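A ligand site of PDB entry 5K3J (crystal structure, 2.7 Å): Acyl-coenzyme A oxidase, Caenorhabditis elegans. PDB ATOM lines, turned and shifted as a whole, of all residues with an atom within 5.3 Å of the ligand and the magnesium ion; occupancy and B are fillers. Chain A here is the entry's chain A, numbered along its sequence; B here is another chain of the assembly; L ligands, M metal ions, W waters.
Water W1 bridges the side-chain carboxylate (OE2) of Glu 398 of chain B (2.6 Å) and an oxygen (O11) of the ligand (2.8 Å). Water W2 lies within hydrogen-bond range of NH2 of Arg 528 and N2 of the ligand.
Residues that only touch the ligand: Tyr 565 of chain B, Arg 341 of chain B, His 394, Met 436, Leu 439 and Val 391. 13 residues have an atom within 4 Å of the ligand: Ser 390, Val 391, His 394, Asn 435, Met 436, Leu 439, Arg 525, Arg 528, Tyr 573, His 340 of chain B, Arg 341 of chain B, Gln 402 of chain B and Tyr 565 of chain B. The nearest printed residue that does not touch the ligand is Met 405 of chain B (4.4 Å).
The guanidinium group of Arg 525 is in salt-bridge range of an oxygen (O7) of the ligand, at 3.6 Å. A ring nitrogen (NE2) of His 340 of chain B lies within hydrogen-bond range of an oxygen (O10) of the ligand, 3.2 Å away. A nitrogen (N4) of the ligand lies close to the side-chain amide oxygen (OD1) of Asn 435 (2.9 Å). An oxygen (O13) of the ligand is in hydrogen-bond range of the side-chain amide oxygen (OE1) of Gln 402 of chain B (2.7 Å). The backbone carbonyl oxygen (O) of Ser 390 is in hydrogen-bond range of a nitrogen (N3) of the ligand (3.2 Å). OH of Tyr 573 sits at hydrogen-bond distance from O1 of the ligand, 2.5 Å away. The guanidinium group of Arg 528 is in salt-bridge range of an oxygen (O7) of the ligand (2.8 Å).
Asp 569 of chain B touches the magnesium ion (OD1 to MG, 3.6 Å). Of the 23 residues printed, 1 comes within 4 Å of the magnesium ion.
The backbone carbonyl oxygen (O) of Ser 390 lies close to the side-chain amide oxygen (OD1) of Asn 435, 3.1 Å away. The backbone carbonyl oxygen of Cys 429 lies within hydrogen-bond range of the side-chain amide nitrogen of Asn 435 (3.2 Å). The backbone NH (N) of His 394 lies within hydrogen-bond range of the side-chain sulfur (SG) of Cys 429 (3.7 Å). OE1 of Gln 402 of chain B lies within hydrogen-bond range of NE of Arg 341 of chain B (2.8 Å).
The magnesium ion is bound by an oxygen (O5) of the ligand (2.0 Å), an oxygen (O8) of the ligand (2.2 Å) and an oxygen (O2) of the ligand (2.3 Å).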
ATOM      1  N   SER A 390     -31.478  18.668 -14.770  1.00  0.00           N
ATOM      2  CA  SER A 390     -30.307  18.390 -13.943  1.00  0.00           C
ATOM      3  C   SER A 390     -30.529  17.188 -13.027  1.00  0.00           C
ATOM      4  O   SER A 390     -29.751  16.234 -13.044  1.00  0.00           O
ATOM      5  CB  SER A 390     -29.932  19.624 -13.116  1.00  0.00           C
ATOM      6  OG  SER A 390     -29.513  20.680 -13.967  1.00  0.00           O
ATOM      7  N   VAL A 391     -31.594  17.246 -12.234  1.00  0.00           N
ATOM      8  CA  VAL A 391     -31.915  16.171 -11.303  1.00  0.00           C
ATOM      9  C   VAL A 391     -32.200  14.866 -12.040  1.00  0.00           C
ATOM     10  O   VAL A 391     -31.709  13.803 -11.648  1.00  0.00           O
ATOM     11  CB  VAL A 391     -33.134  16.521 -10.415  1.00  0.00           C
ATOM     12  CG1 VAL A 391     -33.647  15.291  -9.683  1.00  0.00           C
ATOM     13  CG2 VAL A 391     -32.761  17.615  -9.430  1.00  0.00           C
ATOM     14  N   HIS A 394     -29.047  13.357 -13.683  1.00  0.00           N
ATOM     15  CA  HIS A 394     -28.159  12.903 -12.619  1.00  0.00           C
ATOM     16  C   HIS A 394     -28.648  11.592 -12.012  1.00  0.00           C
ATOM     17  O   HIS A 394     -27.870  10.653 -11.853  1.00  0.00           O
ATOM     18  CB  HIS A 394     -28.045  13.980 -11.539  1.00  0.00           C
ATOM     19  CG  HIS A 394     -27.315  13.530 -10.309  1.00  0.00           C
ATOM     20  ND1 HIS A 394     -25.978  13.221 -10.308  1.00  0.00           N
ATOM     21  CD2 HIS A 394     -27.746  13.341  -9.037  1.00  0.00           C
ATOM     22  CE1 HIS A 394     -25.612  12.861  -9.089  1.00  0.00           C
ATOM     23  NE2 HIS A 394     -26.665  12.919  -8.301  1.00  0.00           N
ATOM     24  N   CYS A 429     -26.079  15.492 -18.413  1.00  0.00           N
ATOM     25  CA  CYS A 429     -25.638  16.229 -17.252  1.00  0.00           C
ATOM     26  C   CYS A 429     -24.730  17.400 -17.645  1.00  0.00           C
ATOM     27  O   CYS A 429     -24.294  18.174 -16.786  1.00  0.00           O
ATOM     28  CB  CYS A 429     -24.894  15.308 -16.287  1.00  0.00           C
ATOM     29  SG  CYS A 429     -25.927  14.063 -15.471  1.00  0.00           S
ATOM     30  N   ASN A 435     -25.100  20.986 -15.325  1.00  0.00           N
ATOM     31  CA  ASN A 435     -26.057  20.671 -14.268  1.00  0.00           C
ATOM     32  C   ASN A 435     -26.002  21.601 -13.052  1.00  0.00           C
ATOM     33  O   ASN A 435     -27.043  22.034 -12.557  1.00  0.00           O
ATOM     34  CB  ASN A 435     -25.859  19.215 -13.800  1.00  0.00           C
ATOM     35  CG  ASN A 435     -26.766  18.247 -14.531  1.00  0.00           C
ATOM     36  OD1 ASN A 435     -27.005  17.140 -14.059  1.00  0.00           O
ATOM     37  ND2 ASN A 435     -27.266  18.664 -15.699  1.00  0.00           N
ATOM     38  N   MET A 436     -24.794  21.890 -12.567  1.00  0.00           N
ATOM     39  CA  MET A 436     -24.627  22.818 -11.449  1.00  0.00           C
ATOM     40  C   MET A 436     -25.138  24.216 -11.790  1.00  0.00           C
ATOM     41  O   MET A 436     -25.817  24.850 -10.990  1.00  0.00           O
ATOM     42  CB  MET A 436     -23.159  22.900 -11.023  1.00  0.00           C
ATOM     43  CG  MET A 436     -22.640  21.695 -10.271  1.00  0.00           C
ATOM     44  SD  MET A 436     -23.687  21.209  -8.873  1.00  0.00           S
ATOM     45  CE  MET A 436     -24.432  19.719  -9.524  1.00  0.00           C
ATOM     46  N   LEU A 439     -28.978  24.097 -12.011  1.00  0.00           N
ATOM     47  CA  LEU A 439     -29.552  24.011 -10.670  1.00  0.00           C
ATOM     48  C   LEU A 439     -29.513  25.384 -10.011  1.00  0.00           C
ATOM     49  O   LEU A 439     -30.398  25.730  -9.225  1.00  0.00           O
ATOM     50  CB  LEU A 439     -28.805  22.981  -9.809  1.00  0.00           C
ATOM     51  CG  LEU A 439     -29.165  21.504  -9.964  1.00  0.00           C
ATOM     52  CD1 LEU A 439     -28.246  20.643  -9.107  1.00  0.00           C
ATOM     53  CD2 LEU A 439     -30.616  21.277  -9.586  1.00  0.00           C
ATOM     54  N   VAL A 521     -24.105  26.225  -2.729  1.00  0.00           N
ATOM     55  CA  VAL A 521     -24.411  24.821  -2.501  1.00  0.00           C
ATOM     56  C   VAL A 521     -25.788  24.640  -1.869  1.00  0.00           C
ATOM     57  O   VAL A 521     -26.558  23.785  -2.302  1.00  0.00           O
ATOM     58  CB  VAL A 521     -23.360  24.153  -1.592  1.00  0.00           C
ATOM     59  CG1 VAL A 521     -23.716  22.688  -1.358  1.00  0.00           C
ATOM     60  CG2 VAL A 521     -21.985  24.261  -2.217  1.00  0.00           C
ATOM     61  N   THR A 524     -28.497  25.016  -4.403  1.00  0.00           N
ATOM     62  CA  THR A 524     -28.684  23.867  -5.272  1.00  0.00           C
ATOM     63  C   THR A 524     -29.403  22.737  -4.541  1.00  0.00           C
ATOM     64  O   THR A 524     -30.098  21.929  -5.167  1.00  0.00           O
ATOM     65  CB  THR A 524     -27.341  23.324  -5.812  1.00  0.00           C
ATOM     66  OG1 THR A 524     -26.486  22.973  -4.710  1.00  0.00           O
ATOM     67  CG2 THR A 524     -26.648  24.362  -6.675  1.00  0.00           C
ATOM     68  N   ARG A 525     -29.239  22.681  -3.229  1.00  0.00           N
ATOM     69  CA  ARG A 525     -29.991  21.721  -2.421  1.00  0.00           C
ATOM     70  C   ARG A 525     -31.465  22.081  -2.483  1.00  0.00           C
ATOM     71  O   ARG A 525     -32.331  21.201  -2.526  1.00  0.00           O
ATOM     72  CB  ARG A 525     -29.504  21.716  -0.974  1.00  0.00           C
ATOM     73  CG  ARG A 525     -28.013  21.445  -0.816  1.00  0.00           C
ATOM     74  CD  ARG A 525     -27.605  21.497   0.651  1.00  0.00           C
ATOM     75  NE  ARG A 525     -26.158  21.393   0.825  1.00  0.00           N
ATOM     76  CZ  ARG A 525     -25.492  20.258   0.841  1.00  0.00           C
ATOM     77  NH1 ARG A 525     -26.122  19.103   0.678  1.00  0.00           N
ATOM     78  NH2 ARG A 525     -24.175  20.259   1.011  1.00  0.00           N
ATOM     79  N   ARG A 528     -32.903  21.075  -6.110  1.00  0.00           N
ATOM     80  CA  ARG A 528     -33.129  19.631  -6.172  1.00  0.00           C
ATOM     81  C   ARG A 528     -34.405  19.214  -5.437  1.00  0.00           C
ATOM     82  O   ARG A 528     -35.196  18.431  -5.964  1.00  0.00           O
ATOM     83  CB  ARG A 528     -31.935  18.868  -5.591  1.00  0.00           C
ATOM     84  CG  ARG A 528     -30.808  18.625  -6.590  1.00  0.00           C
ATOM     85  CD  ARG A 528     -29.742  17.708  -6.013  1.00  0.00           C
ATOM     86  NE  ARG A 528     -28.605  18.445  -5.460  1.00  0.00           N
ATOM     87  CZ  ARG A 528     -28.475  18.759  -4.178  1.00  0.00           C
ATOM     88  NH1 ARG A 528     -29.397  18.398  -3.307  1.00  0.00           N
ATOM     89  NH2 ARG A 528     -27.413  19.435  -3.765  1.00  0.00           N
ATOM     90  N   ARG A 532     -37.871  17.565  -7.240  1.00  0.00           N
ATOM     91  CA  ARG A 532     -38.224  16.222  -6.835  1.00  0.00           C
ATOM     92  C   ARG A 532     -39.669  16.206  -6.374  1.00  0.00           C
ATOM     93  O   ARG A 532     -40.394  15.233  -6.580  1.00  0.00           O
ATOM     94  CB  ARG A 532     -37.295  15.718  -5.718  1.00  0.00           C
ATOM     95  CG  ARG A 532     -35.903  15.352  -6.204  1.00  0.00           C
ATOM     96  CD  ARG A 532     -35.495  13.975  -5.712  1.00  0.00           C
ATOM     97  NE  ARG A 532     -34.291  14.033  -4.890  1.00  0.00           N
ATOM     98  CZ  ARG A 532     -33.741  12.967  -4.316  1.00  0.00           C
ATOM     99  NH1 ARG A 532     -34.282  11.766  -4.474  1.00  0.00           N
ATOM    100  NH2 ARG A 532     -32.650  13.103  -3.584  1.00  0.00           N
ATOM    101  N   ASP A 569     -34.231   8.898   0.881  1.00  0.00           N
ATOM    102  CA  ASP A 569     -33.015   9.435   0.279  1.00  0.00           C
ATOM    103  C   ASP A 569     -32.769  10.873   0.731  1.00  0.00           C
ATOM    104  O   ASP A 569     -31.650  11.375   0.656  1.00  0.00           O
ATOM    105  CB  ASP A 569     -33.090   9.362  -1.241  1.00  0.00           C
ATOM    106  CG  ASP A 569     -31.759   9.672  -1.915  1.00  0.00           C
ATOM    107  OD1 ASP A 569     -30.728   9.149  -1.453  1.00  0.00           O
ATOM    108  OD2 ASP A 569     -31.755  10.435  -2.901  1.00  0.00           O
ATOM    109  N   VAL A 570     -33.831  11.518   1.197  1.00  0.00           N
ATOM    110  CA  VAL A 570     -33.763  12.916   1.628  1.00  0.00           C
ATOM    111  C   VAL A 570     -34.200  13.093   3.072  1.00  0.00           C
ATOM    112  O   VAL A 570     -34.613  14.180   3.477  1.00  0.00           O
ATOM    113  CB  VAL A 570     -34.648  13.823   0.729  1.00  0.00           C
ATOM    114  CG1 VAL A 570     -34.158  13.787  -0.706  1.00  0.00           C
ATOM    115  CG2 VAL A 570     -36.103  13.393   0.822  1.00  0.00           C
ATOM    116  N   TYR A 573     -33.434  16.021   5.452  1.00  0.00           N
ATOM    117  CA  TYR A 573     -34.291  17.197   5.345  1.00  0.00           C
ATOM    118  C   TYR A 573     -35.675  16.937   5.938  1.00  0.00           C
ATOM    119  O   TYR A 573     -36.339  17.845   6.428  1.00  0.00           O
ATOM    120  CB  TYR A 573     -34.428  17.635   3.879  1.00  0.00           C
ATOM    121  CG  TYR A 573     -33.125  18.035   3.238  1.00  0.00           C
ATOM    122  CD1 TYR A 573     -32.376  19.076   3.760  1.00  0.00           C
ATOM    123  CD2 TYR A 573     -32.664  17.395   2.090  1.00  0.00           C
ATOM    124  CE1 TYR A 573     -31.183  19.461   3.164  1.00  0.00           C
ATOM    125  CE2 TYR A 573     -31.478  17.768   1.495  1.00  0.00           C
ATOM    126  CZ  TYR A 573     -30.735  18.803   2.038  1.00  0.00           C
ATOM    127  OH  TYR A 573     -29.553  19.178   1.452  1.00  0.00           O
ATOM    128  N   HIS B 340     -16.871  22.138  -4.185  1.00  0.00           N
ATOM    129  CA  HIS B 340     -17.719  21.154  -3.525  1.00  0.00           C
ATOM    130  C   HIS B 340     -17.709  19.817  -4.262  1.00  0.00           C
ATOM    131  O   HIS B 340     -17.700  18.766  -3.632  1.00  0.00           O
ATOM    132  CB  HIS B 340     -19.159  21.658  -3.430  1.00  0.00           C
ATOM    133  CG  HIS B 340     -20.110  20.679  -2.825  1.00  0.00           C
ATOM    134  ND1 HIS B 340     -19.947  20.194  -1.549  1.00  0.00           N
ATOM    135  CD2 HIS B 340     -21.206  20.073  -3.327  1.00  0.00           C
ATOM    136  CE1 HIS B 340     -20.921  19.345  -1.277  1.00  0.00           C
ATOM    137  NE2 HIS B 340     -21.699  19.252  -2.344  1.00  0.00           N
ATOM    138  N   ARG B 341     -17.712  19.891  -5.577  1.00  0.00           N
ATOM    139  CA  ARG B 341     -17.812  18.679  -6.393  1.00  0.00           C
ATOM    140  C   ARG B 341     -16.437  18.067  -6.678  1.00  0.00           C
ATOM    141  O   ARG B 341     -16.325  17.091  -7.419  1.00  0.00           O
ATOM    142  CB  ARG B 341     -18.543  18.973  -7.706  1.00  0.00           C
ATOM    143  CG  ARG B 341     -17.690  19.600  -8.798  1.00  0.00           C
ATOM    144  CD  ARG B 341     -18.537  19.922 -10.024  1.00  0.00           C
ATOM    145  NE  ARG B 341     -19.391  18.796 -10.423  1.00  0.00           N
ATOM    146  CZ  ARG B 341     -20.281  18.862 -11.400  1.00  0.00           C
ATOM    147  NH1 ARG B 341     -20.447  19.985 -12.082  1.00  0.00           N
ATOM    148  NH2 ARG B 341     -21.025  17.793 -11.690  1.00  0.00           N
ATOM    149  N   GLU B 398     -18.140   7.617  -8.116  1.00  0.00           N
ATOM    150  CA  GLU B 398     -18.934   8.829  -7.960  1.00  0.00           C
ATOM    151  C   GLU B 398     -18.057  10.059  -8.158  1.00  0.00           C
ATOM    152  O   GLU B 398     -18.414  10.983  -8.880  1.00  0.00           O
ATOM    153  CB  GLU B 398     -19.580   8.844  -6.564  1.00  0.00           C
ATOM    154  CG  GLU B 398     -20.899   9.589  -6.490  1.00  0.00           C
ATOM    155  CD  GLU B 398     -21.554   9.453  -5.126  1.00  0.00           C
ATOM    156  OE1 GLU B 398     -21.245   8.476  -4.410  1.00  0.00           O
ATOM    157  OE2 GLU B 398     -22.371  10.331  -4.772  1.00  0.00           O
ATOM    158  N   GLN B 402     -17.771  13.101 -11.192  1.00  0.00           N
ATOM    159  CA  GLN B 402     -17.822  14.471 -10.715  1.00  0.00           C
ATOM    160  C   GLN B 402     -16.614  15.245 -11.213  1.00  0.00           C
ATOM    161  O   GLN B 402     -16.725  16.415 -11.559  1.00  0.00           O
ATOM    162  CB  GLN B 402     -17.886  14.529  -9.194  1.00  0.00           C
ATOM    163  CG  GLN B 402     -19.241  14.185  -8.611  1.00  0.00           C
ATOM    164  CD  GLN B 402     -20.344  15.091  -9.134  1.00  0.00           C
ATOM    165  OE1 GLN B 402     -20.156  16.302  -9.297  1.00  0.00           O
ATOM    166  NE2 GLN B 402     -21.503  14.507  -9.411  1.00  0.00           N
ATOM    167  N   MET B 405     -17.366  15.677 -15.206  1.00  0.00           N
ATOM    168  CA  MET B 405     -18.392  16.692 -15.445  1.00  0.00           C
ATOM    169  C   MET B 405     -17.893  18.076 -15.039  1.00  0.00           C
ATOM    170  O   MET B 405     -18.299  19.079 -15.625  1.00  0.00           O
ATOM    171  CB  MET B 405     -19.676  16.345 -14.686  1.00  0.00           C
ATOM    172  CG  MET B 405     -20.383  15.089 -15.203  1.00  0.00           C
ATOM    173  SD  MET B 405     -21.955  14.744 -14.377  1.00  0.00           S
ATOM    174  CE  MET B 405     -21.391  14.088 -12.808  1.00  0.00           C
ATOM    175  N   TYR B 565     -17.913  16.517   5.383  1.00  0.00           N
ATOM    176  CA  TYR B 565     -18.639  16.170   4.169  1.00  0.00           C
ATOM    177  C   TYR B 565     -19.222  14.769   4.334  1.00  0.00           C
ATOM    178  O   TYR B 565     -20.389  14.537   3.997  1.00  0.00           O
ATOM    179  CB  TYR B 565     -17.728  16.248   2.940  1.00  0.00           C
ATOM    180  CG  TYR B 565     -18.413  15.843   1.658  1.00  0.00           C
ATOM    181  CD1 TYR B 565     -19.197  16.746   0.948  1.00  0.00           C
ATOM    182  CD2 TYR B 565     -18.278  14.554   1.152  1.00  0.00           C
ATOM    183  CE1 TYR B 565     -19.821  16.377  -0.228  1.00  0.00           C
ATOM    184  CE2 TYR B 565     -18.901  14.185  -0.025  1.00  0.00           C
ATOM    185  CZ  TYR B 565     -19.675  15.097  -0.710  1.00  0.00           C
ATOM    186  OH  TYR B 565     -20.293  14.733  -1.874  1.00  0.00           O
ATOM    187  N   LEU B 568     -22.226  14.685   6.862  1.00  0.00           N
ATOM    188  CA  LEU B 568     -23.448  15.298   6.329  1.00  0.00           C
ATOM    189  C   LEU B 568     -24.096  14.406   5.265  1.00  0.00           C
ATOM    190  O   LEU B 568     -25.306  14.440   5.076  1.00  0.00           O
ATOM    191  CB  LEU B 568     -23.124  16.676   5.758  1.00  0.00           C
ATOM    192  CG  LEU B 568     -24.273  17.479   5.141  1.00  0.00           C
ATOM    193  CD1 LEU B 568     -25.463  17.554   6.089  1.00  0.00           C
ATOM    194  CD2 LEU B 568     -23.793  18.869   4.745  1.00  0.00           C
ATOM    195  N   ASP B 569     -23.279  13.596   4.603  1.00  0.00           N
ATOM    196  CA  ASP B 569     -23.772  12.642   3.621  1.00  0.00           C
ATOM    197  C   ASP B 569     -24.531  11.520   4.333  1.00  0.00           C
ATOM    198  O   ASP B 569     -25.318  10.793   3.714  1.00  0.00           O
ATOM    199  CB  ASP B 569     -22.626  12.080   2.779  1.00  0.00           C
ATOM    200  CG  ASP B 569     -23.115  11.256   1.609  1.00  0.00           C
ATOM    201  OD1 ASP B 569     -24.163  11.607   1.028  1.00  0.00           O
ATOM    202  OD2 ASP B 569     -22.441  10.250   1.271  1.00  0.00           O
HETATM  203  P1  LIG L   1     -28.562  16.381  -0.772  1.00  0.00           P
HETATM  204  O1  LIG L   1     -29.305  17.677  -0.582  1.00  0.00           O
HETATM  205  O2  LIG L   1     -27.310  16.252   0.074  1.00  0.00           O
HETATM  206  O3  LIG L   1     -29.442  15.153  -0.788  1.00  0.00           O
HETATM  207  P2  LIG L   1     -26.925  15.433  -2.847  1.00  0.00           P
HETATM  208  O4  LIG L   1     -27.563  14.625  -3.950  1.00  0.00           O
HETATM  209  O5  LIG L   1     -26.271  14.732  -1.685  1.00  0.00           O
HETATM  210  O6  LIG L   1     -28.003  16.493  -2.282  1.00  0.00           O
HETATM  211  P3  LIG L   1     -24.754  17.165  -2.610  1.00  0.00           P
HETATM  212  O7  LIG L   1     -24.955  18.654  -2.719  1.00  0.00           O
HETATM  213  O8  LIG L   1     -24.765  16.504  -1.251  1.00  0.00           O
HETATM  214  O9  LIG L   1     -25.868  16.439  -3.525  1.00  0.00           O
HETATM  215  O10 LIG L   1     -23.394  16.769  -3.359  1.00  0.00           O
HETATM  216  C1  LIG L   1     -23.053  15.387  -3.552  1.00  0.00           C
HETATM  217  C2  LIG L   1     -22.420  15.288  -4.933  1.00  0.00           C
HETATM  218  O11 LIG L   1     -23.414  15.020  -5.924  1.00  0.00           O
HETATM  219  C3  LIG L   1     -21.761  16.610  -5.280  1.00  0.00           C
HETATM  220  O12 LIG L   1     -20.390  16.389  -5.611  1.00  0.00           O
HETATM  221  C4  LIG L   1     -22.517  17.125  -6.493  1.00  0.00           C
HETATM  222  O13 LIG L   1     -21.639  17.679  -7.467  1.00  0.00           O
HETATM  223  C5  LIG L   1     -23.252  15.911  -7.031  1.00  0.00           C
HETATM  224  N1  LIG L   1     -24.565  16.266  -7.615  1.00  0.00           N
HETATM  225  C6  LIG L   1     -25.682  16.505  -6.923  1.00  0.00           C
HETATM  226  N2  LIG L   1     -26.727  16.797  -7.745  1.00  0.00           N
HETATM  227  C7  LIG L   1     -26.268  16.738  -9.008  1.00  0.00           C
HETATM  228  C8  LIG L   1     -26.836  16.940 -10.363  1.00  0.00           C
HETATM  229  N3  LIG L   1     -28.143  17.273 -10.536  1.00  0.00           N
HETATM  230  N4  LIG L   1     -26.001  16.775 -11.416  1.00  0.00           N
HETATM  231  C9  LIG L   1     -24.705  16.448 -11.250  1.00  0.00           C
HETATM  232  N5  LIG L   1     -24.126  16.257 -10.061  1.00  0.00           N
HETATM  233  C10 LIG L   1     -24.838  16.388  -8.924  1.00  0.00           C
HETATM  234 MG    MG M   1     -25.442  14.874   0.106  1.00  0.00          MG
HETATM  235  O   HOH W   1     -23.158  12.290  -6.323  1.00  0.00           O
HETATM  236  O   HOH W   2     -26.106  19.393  -6.022  1.00  0.00           O
